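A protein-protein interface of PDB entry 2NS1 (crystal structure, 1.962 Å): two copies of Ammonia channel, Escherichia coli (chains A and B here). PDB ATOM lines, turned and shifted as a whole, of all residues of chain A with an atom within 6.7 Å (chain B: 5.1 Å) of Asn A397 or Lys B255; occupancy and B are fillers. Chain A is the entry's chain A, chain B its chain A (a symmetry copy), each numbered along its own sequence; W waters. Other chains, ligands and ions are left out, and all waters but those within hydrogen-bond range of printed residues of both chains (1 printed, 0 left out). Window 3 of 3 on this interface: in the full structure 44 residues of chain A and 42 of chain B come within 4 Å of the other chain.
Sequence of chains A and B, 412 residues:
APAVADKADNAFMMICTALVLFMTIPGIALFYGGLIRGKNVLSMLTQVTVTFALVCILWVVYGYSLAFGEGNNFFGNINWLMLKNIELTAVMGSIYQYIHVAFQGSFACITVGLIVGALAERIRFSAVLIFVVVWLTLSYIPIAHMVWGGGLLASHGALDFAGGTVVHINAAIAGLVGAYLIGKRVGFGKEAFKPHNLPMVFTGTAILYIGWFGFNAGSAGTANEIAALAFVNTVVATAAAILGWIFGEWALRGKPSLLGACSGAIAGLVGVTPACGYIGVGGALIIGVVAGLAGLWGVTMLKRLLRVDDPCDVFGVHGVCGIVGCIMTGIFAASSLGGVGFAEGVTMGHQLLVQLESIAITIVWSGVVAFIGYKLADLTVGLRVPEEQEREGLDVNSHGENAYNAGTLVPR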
ATOM      1  N   GLU A 388      19.667  23.189  11.489  1.00  0.00           N
ATOM      2  CA  GLU A 388      18.646  23.885  12.272  1.00  0.00           C
ATOM      3  C   GLU A 388      17.610  22.913  12.830  1.00  0.00           C
ATOM      4  O   GLU A 388      17.028  23.166  13.881  1.00  0.00           O
ATOM      5  CB  GLU A 388      17.963  25.017  11.495  1.00  0.00           C
ATOM      6  CG  GLU A 388      17.511  26.178  12.439  1.00  0.00           C
ATOM      7  CD  GLU A 388      18.664  26.813  13.288  1.00  0.00           C
ATOM      8  OE1 GLU A 388      19.846  26.805  12.852  1.00  0.00           O
ATOM      9  OE2 GLU A 388      18.380  27.321  14.404  1.00  0.00           O
ATOM     10  N   GLN A 389      17.384  21.814  12.126  1.00  0.00           N
ATOM     11  CA  GLN A 389      16.547  20.739  12.660  1.00  0.00           C
ATOM     12  C   GLN A 389      17.221  20.119  13.879  1.00  0.00           C
ATOM     13  O   GLN A 389      16.561  19.816  14.871  1.00  0.00           O
ATOM     14  CB  GLN A 389      16.286  19.688  11.601  1.00  0.00           C
ATOM     15  CG  GLN A 389      15.402  20.160  10.455  1.00  0.00           C
ATOM     16  CD  GLN A 389      14.924  19.005   9.575  1.00  0.00           C
ATOM     17  OE1 GLN A 389      14.926  17.846   9.990  1.00  0.00           O
ATOM     18  NE2 GLN A 389      14.512  19.320   8.356  1.00  0.00           N
ATOM     19  N   GLU A 390      18.544  19.960  13.814  1.00  0.00           N
ATOM     20  CA  GLU A 390      19.307  19.400  14.918  1.00  0.00           C
ATOM     21  C   GLU A 390      19.240  20.291  16.164  1.00  0.00           C
ATOM     22  O   GLU A 390      19.089  19.805  17.290  1.00  0.00           O
ATOM     23  CB  GLU A 390      20.757  19.158  14.490  1.00  0.00           C
ATOM     24  CG  GLU A 390      21.593  18.543  15.582  1.00  0.00           C
ATOM     25  CD  GLU A 390      23.033  18.245  15.187  1.00  0.00           C
ATOM     26  OE1 GLU A 390      23.362  18.308  13.983  1.00  0.00           O
ATOM     27  OE2 GLU A 390      23.826  17.959  16.109  1.00  0.00           O
ATOM     28  N   ARG A 391      19.319  21.605  15.964  1.00  0.00           N
ATOM     29  CA  ARG A 391      19.210  22.577  17.072  1.00  0.00           C
ATOM     30  C   ARG A 391      17.849  22.611  17.743  1.00  0.00           C
ATOM     31  O   ARG A 391      17.753  22.767  18.964  1.00  0.00           O
ATOM     32  CB  ARG A 391      19.472  24.001  16.560  1.00  0.00           C
ATOM     33  CG  ARG A 391      20.875  24.240  16.145  1.00  0.00           C
ATOM     34  CD  ARG A 391      21.684  24.523  17.361  1.00  0.00           C
ATOM     35  NE  ARG A 391      23.059  24.897  17.069  1.00  0.00           N
ATOM     36  CZ  ARG A 391      23.980  25.011  18.016  1.00  0.00           C
ATOM     37  NH1 ARG A 391      23.659  24.756  19.279  1.00  0.00           N
ATOM     38  NH2 ARG A 391      25.220  25.364  17.700  1.00  0.00           N
ATOM     39  N   GLU A 392      16.810  22.516  16.932  1.00  0.00           N
ATOM     40  CA  GLU A 392      15.435  22.512  17.415  1.00  0.00           C
ATOM     41  C   GLU A 392      15.098  21.172  18.063  1.00  0.00           C
ATOM     42  O   GLU A 392      14.272  21.104  18.948  1.00  0.00           O
ATOM     43  CB  GLU A 392      14.481  22.760  16.255  1.00  0.00           C
ATOM     44  CG  GLU A 392      14.575  24.176  15.688  1.00  0.00           C
ATOM     45  CD  GLU A 392      13.938  24.324  14.307  1.00  0.00           C
ATOM     46  OE1 GLU A 392      13.428  23.312  13.762  1.00  0.00           O
ATOM     47  OE2 GLU A 392      13.956  25.464  13.768  1.00  0.00           O
ATOM     48  N   GLY A 393      15.720  20.116  17.570  1.00  0.00           N
ATOM     49  CA  GLY A 393      15.536  18.769  18.095  1.00  0.00           C
ATOM     50  C   GLY A 393      14.813  17.952  17.054  1.00  0.00           C
ATOM     51  O   GLY A 393      13.954  18.466  16.318  1.00  0.00           O
ATOM     52  N   LEU A 394      15.156  16.674  16.989  1.00  0.00           N
ATOM     53  CA  LEU A 394      14.523  15.749  16.060  1.00  0.00           C
ATOM     54  C   LEU A 394      13.060  15.437  16.371  1.00  0.00           C
ATOM     55  O   LEU A 394      12.317  15.066  15.472  1.00  0.00           O
ATOM     56  CB  LEU A 394      15.311  14.434  16.001  1.00  0.00           C
ATOM     57  CG  LEU A 394      16.794  14.480  15.608  1.00  0.00           C
ATOM     58  CD1 LEU A 394      17.350  13.058  15.539  1.00  0.00           C
ATOM     59  CD2 LEU A 394      17.011  15.187  14.291  1.00  0.00           C
ATOM     60  N   ASP A 395      12.622  15.561  17.616  1.00  0.00           N
ATOM     61  CA  ASP A 395      11.245  15.135  17.927  1.00  0.00           C
ATOM     62  C   ASP A 395      10.257  15.986  17.131  1.00  0.00           C
ATOM     63  O   ASP A 395       9.389  15.467  16.439  1.00  0.00           O
ATOM     64  CB  ASP A 395      10.938  15.237  19.420  1.00  0.00           C
ATOM     65  CG  ASP A 395      11.754  14.244  20.270  1.00  0.00           C
ATOM     66  OD1 ASP A 395      12.473  13.415  19.669  1.00  0.00           O
ATOM     67  OD2 ASP A 395      11.674  14.310  21.536  1.00  0.00           O
ATOM     68  N   VAL A 396      10.397  17.300  17.210  1.00  0.00           N
ATOM     69  CA  VAL A 396       9.450  18.173  16.504  1.00  0.00           C
ATOM     70  C   VAL A 396       9.614  18.054  15.004  1.00  0.00           C
ATOM     71  O   VAL A 396       8.630  17.955  14.271  1.00  0.00           O
ATOM     72  CB  VAL A 396       9.543  19.639  16.954  1.00  0.00           C
ATOM     73  CG1 VAL A 396       8.943  19.770  18.352  1.00  0.00           C
ATOM     74  CG2 VAL A 396      10.996  20.161  16.895  1.00  0.00           C
ATOM     75  N   ASN A 397      10.861  18.023  14.557  1.00  0.00           N
ATOM     76  CA  ASN A 397      11.180  18.050  13.138  1.00  0.00           C
ATOM     77  C   ASN A 397      10.938  16.729  12.412  1.00  0.00           C
ATOM     78  O   ASN A 397      10.342  16.710  11.342  1.00  0.00           O
ATOM     79  CB  ASN A 397      12.628  18.557  12.953  1.00  0.00           C
ATOM     80  CG  ASN A 397      12.722  20.073  13.057  1.00  0.00           C
ATOM     81  OD1 ASN A 397      12.178  20.781  12.214  1.00  0.00           O
ATOM     82  ND2 ASN A 397      13.367  20.573  14.104  1.00  0.00           N
ATOM     83  N   SER A 398      11.379  15.611  12.983  1.00  0.00           N
ATOM     84  CA  SER A 398      11.197  14.312  12.320  1.00  0.00           C
ATOM     85  C   SER A 398       9.877  13.657  12.659  1.00  0.00           C
ATOM     86  O   SER A 398       9.392  12.828  11.905  1.00  0.00           O
ATOM     87  CB  SER A 398      12.347  13.352  12.677  1.00  0.00           C
ATOM     88  OG  SER A 398      13.595  13.904  12.305  1.00  0.00           O
ATOM     89  N   HIS A 399       9.310  14.007  13.813  1.00  0.00           N
ATOM     90  CA  HIS A 399       8.176  13.262  14.358  1.00  0.00           C
ATOM     91  C   HIS A 399       6.914  14.075  14.681  1.00  0.00           C
ATOM     92  O   HIS A 399       5.837  13.491  14.909  1.00  0.00           O
ATOM     93  CB  HIS A 399       8.666  12.454  15.574  1.00  0.00           C
ATOM     94  CG  HIS A 399       9.750  11.486  15.213  1.00  0.00           C
ATOM     95  ND1 HIS A 399       9.552  10.473  14.306  1.00  0.00           N
ATOM     96  CD2 HIS A 399      11.050  11.417  15.577  1.00  0.00           C
ATOM     97  CE1 HIS A 399      10.683   9.817  14.125  1.00  0.00           C
ATOM     98  NE2 HIS A 399      11.611  10.374  14.879  1.00  0.00           N
ATOM     99  N   GLY A 400       7.014  15.397  14.686  1.00  0.00           N
ATOM    100  CA  GLY A 400       5.828  16.227  14.929  1.00  0.00           C
ATOM    101  C   GLY A 400       5.272  16.154  16.345  1.00  0.00           C
ATOM    102  O   GLY A 400       4.089  16.394  16.569  1.00  0.00           O
ATOM    103  N   GLU A 401       6.122  15.849  17.320  1.00  0.00           N
ATOM    104  CA  GLU A 401       5.660  15.688  18.690  1.00  0.00           C
ATOM    105  C   GLU A 401       6.680  16.242  19.670  1.00  0.00           C
ATOM    106  O   GLU A 401       7.877  16.300  19.387  1.00  0.00           O
ATOM    107  CB  GLU A 401       5.320  14.202  18.951  1.00  0.00           C
ATOM    108  CG  GLU A 401       4.121  13.698  18.059  1.00  0.00           C
ATOM    109  CD  GLU A 401       3.507  12.309  18.371  1.00  0.00           C
ATOM    110  OE1 GLU A 401       4.242  11.409  18.841  1.00  0.00           O
ATOM    111  OE2 GLU A 401       2.285  12.097  18.035  1.00  0.00           O
ATOM    112  N   GLU B 249       0.402   7.159   8.352  1.00  0.00           N
ATOM    113  CA  GLU B 249       0.600   8.449   8.992  1.00  0.00           C
ATOM    114  C   GLU B 249       1.611   9.260   8.186  1.00  0.00           C
ATOM    115  O   GLU B 249       1.390  10.431   7.873  1.00  0.00           O
ATOM    116  CB  GLU B 249       1.103   8.164  10.415  1.00  0.00           C
ATOM    117  CG  GLU B 249       1.312   9.295  11.322  1.00  0.00           C
ATOM    118  CD  GLU B 249       1.863   8.816  12.662  1.00  0.00           C
ATOM    119  OE1 GLU B 249       2.800   7.985  12.674  1.00  0.00           O
ATOM    120  OE2 GLU B 249       1.332   9.239  13.690  1.00  0.00           O
ATOM    121  N   TRP B 250       2.699   8.612   7.807  1.00  0.00           N
ATOM    122  CA  TRP B 250       3.792   9.291   7.135  1.00  0.00           C
ATOM    123  C   TRP B 250       3.276   9.796   5.780  1.00  0.00           C
ATOM    124  O   TRP B 250       3.479  10.949   5.412  1.00  0.00           O
ATOM    125  CB  TRP B 250       4.954   8.319   6.925  1.00  0.00           C
ATOM    126  CG  TRP B 250       6.300   8.940   6.735  1.00  0.00           C
ATOM    127  CD1 TRP B 250       6.585  10.209   6.325  1.00  0.00           C
ATOM    128  CD2 TRP B 250       7.559   8.281   6.912  1.00  0.00           C
ATOM    129  NE1 TRP B 250       7.951  10.391   6.264  1.00  0.00           N
ATOM    130  CE2 TRP B 250       8.567   9.217   6.621  1.00  0.00           C
ATOM    131  CE3 TRP B 250       7.927   6.989   7.305  1.00  0.00           C
ATOM    132  CZ2 TRP B 250       9.916   8.902   6.710  1.00  0.00           C
ATOM    133  CZ3 TRP B 250       9.256   6.678   7.384  1.00  0.00           C
ATOM    134  CH2 TRP B 250      10.239   7.630   7.097  1.00  0.00           C
ATOM    135  N   ARG B 253      -0.142  12.293   6.524  1.00  0.00           N
ATOM    136  CA  ARG B 253       0.035  13.460   7.406  1.00  0.00           C
ATOM    137  C   ARG B 253       1.438  14.060   7.341  1.00  0.00           C
ATOM    138  O   ARG B 253       1.657  15.183   7.770  1.00  0.00           O
ATOM    139  CB  ARG B 253      -0.324  13.080   8.834  1.00  0.00           C
ATOM    140  CG  ARG B 253      -1.770  12.631   8.985  1.00  0.00           C
ATOM    141  CD  ARG B 253      -1.972  11.661  10.145  1.00  0.00           C
ATOM    142  NE  ARG B 253      -1.490  12.197  11.421  1.00  0.00           N
ATOM    143  CZ  ARG B 253      -1.799  11.709  12.627  1.00  0.00           C
ATOM    144  NH1 ARG B 253      -2.610  10.661  12.770  1.00  0.00           N
ATOM    145  NH2 ARG B 253      -1.294  12.286  13.708  1.00  0.00           N
ATOM    146  N   GLY B 254       2.387  13.312   6.797  1.00  0.00           N
ATOM    147  CA  GLY B 254       3.687  13.852   6.487  1.00  0.00           C
ATOM    148  C   GLY B 254       4.809  13.418   7.394  1.00  0.00           C
ATOM    149  O   GLY B 254       5.975  13.615   7.047  1.00  0.00           O
ATOM    150  N   LYS B 255       4.482  12.842   8.553  1.00  0.00           N
ATOM    151  CA  LYS B 255       5.530  12.417   9.509  1.00  0.00           C
ATOM    152  C   LYS B 255       5.169  11.141  10.263  1.00  0.00           C
ATOM    153  O   LYS B 255       4.035  10.974  10.684  1.00  0.00           O
ATOM    154  CB  LYS B 255       5.795  13.513  10.537  1.00  0.00           C
ATOM    155  CG  LYS B 255       6.465  14.742   9.963  1.00  0.00           C
ATOM    156  CD  LYS B 255       6.706  15.783  11.027  1.00  0.00           C
ATOM    157  CE  LYS B 255       7.253  17.078  10.420  1.00  0.00           C
ATOM    158  NZ  LYS B 255       7.474  18.126  11.448  1.00  0.00           N
ATOM    159  N   PRO B 256       6.161  10.277  10.501  1.00  0.00           N
ATOM    160  CA  PRO B 256       5.981   9.114  11.360  1.00  0.00           C
ATOM    161  C   PRO B 256       6.174   9.561  12.820  1.00  0.00           C
ATOM    162  O   PRO B 256       7.105  10.310  13.103  1.00  0.00           O
ATOM    163  CB  PRO B 256       7.099   8.197  10.914  1.00  0.00           C
ATOM    164  CG  PRO B 256       8.213   9.134  10.522  1.00  0.00           C
ATOM    165  CD  PRO B 256       7.556  10.404  10.032  1.00  0.00           C
ATOM    166  N   SER B 257       5.266   9.173  13.718  1.00  0.00           N
ATOM    167  CA  SER B 257       5.264   9.715  15.075  1.00  0.00           C
ATOM    168  C   SER B 257       5.402   8.619  16.108  1.00  0.00           C
ATOM    169  O   SER B 257       5.079   7.471  15.835  1.00  0.00           O
ATOM    170  CB  SER B 257       3.995  10.512  15.339  1.00  0.00           C
ATOM    171  OG  SER B 257       2.859   9.687  15.525  1.00  0.00           O
HETATM  172  O   HOH W   1      -0.090  10.407  16.344  1.00  0.00           O
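The side-chain amino group of Lys B255 is in hydrogen-bond range of the backbone carbonyl oxygen of Asn A397, at 3.2 Å. The side-chain amino group (NZ) of Lys B255 sits at hydrogen-bond distance from the backbone carbonyl oxygen (O) of Val A396. ND1 of His A399 sits at hydrogen-bond distance from O of Pro B256 (2.7 Å).
The backbone carbonyl oxygen of Gln A389 sits at hydrogen-bond distance from the side-chain amide nitrogen of Asn A397 (3.4 Å). The side-chain carboxylate of Glu B249 lies within hydrogen-bond range of the side-chain hydroxyl of Ser B257, 2.4 Å away. The backbone NH (N) of Val A396 is in hydrogen-bond range of the backbone carbonyl oxygen (O) of Glu A401 (3.5 Å). O of Asp A395 sits at hydrogen-bond distance from N of Gly A400, at 3.0 Å. O of Gly A393 sits at hydrogen-bond distance from ND2 of Asn A397 (3.1 Å). O of Asp A395 sits at hydrogen-bond distance from N of Glu A401, 3.4 Å away.
CB of Lys B255 touches O of Ser A398 (3.9 Å). Ser A398 touches Pro B256 (O to CD, 3.6 Å). His A399 touches Ser B257. CD of Lys B255 touches N of Gly A400 (3.7 Å). OE2 of Glu A401 touches OG of Ser B257 (3.5 Å).
Leu A394 touches none of the printed residues of chain B. Printed residues of chain B within 4 Å of Val A396: Lys B255. Asn A397 touches one residue of chain B. Printed residues of chain B within 4 Å of Ser A398: Lys B255 (3.9 Å) and Pro B256 (3.6 Å). Printed residues of chain B within 4 Å of Gly A400: Lys B255. Lys B255 touches four residues of chain A. Of the printed residues of chain A, Ser B257 touches His A399 and Glu A401. The nearest residue of chain A that does not touch Lys B255 is His A399 (4.04 Å).
Of the 14 printed residues of chain A, 6 touch a printed residue of chain B. Printed residues of chain A that touch a printed residue of chain B: Val A396, Asn A397, Ser A398, His A399, Gly A400 and Glu A401. Hydrophobic or aromatic side chains of chain A within 4 Å of the printed part of chain B: His A399. Of the 7 printed residues of chain B, 3 touch a printed residue of chain A. Hydrophobic or aromatic side chains of chain B within 4 Å of the printed part of chain A: Pro B256. Among the printed residues, no Asp or Glu carboxylate lies within 4 Å of a Lys or Arg side-chain nitrogen of the other chain.
No position is printed for both chains.
Water W1 lies within hydrogen-bond range of OG of Ser B257 (3.1 Å), OE2 of Glu B249 (3.2 Å), OE2 of Glu A401 (3.4 Å) and NH2 of Arg B253 (3.5 Å).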
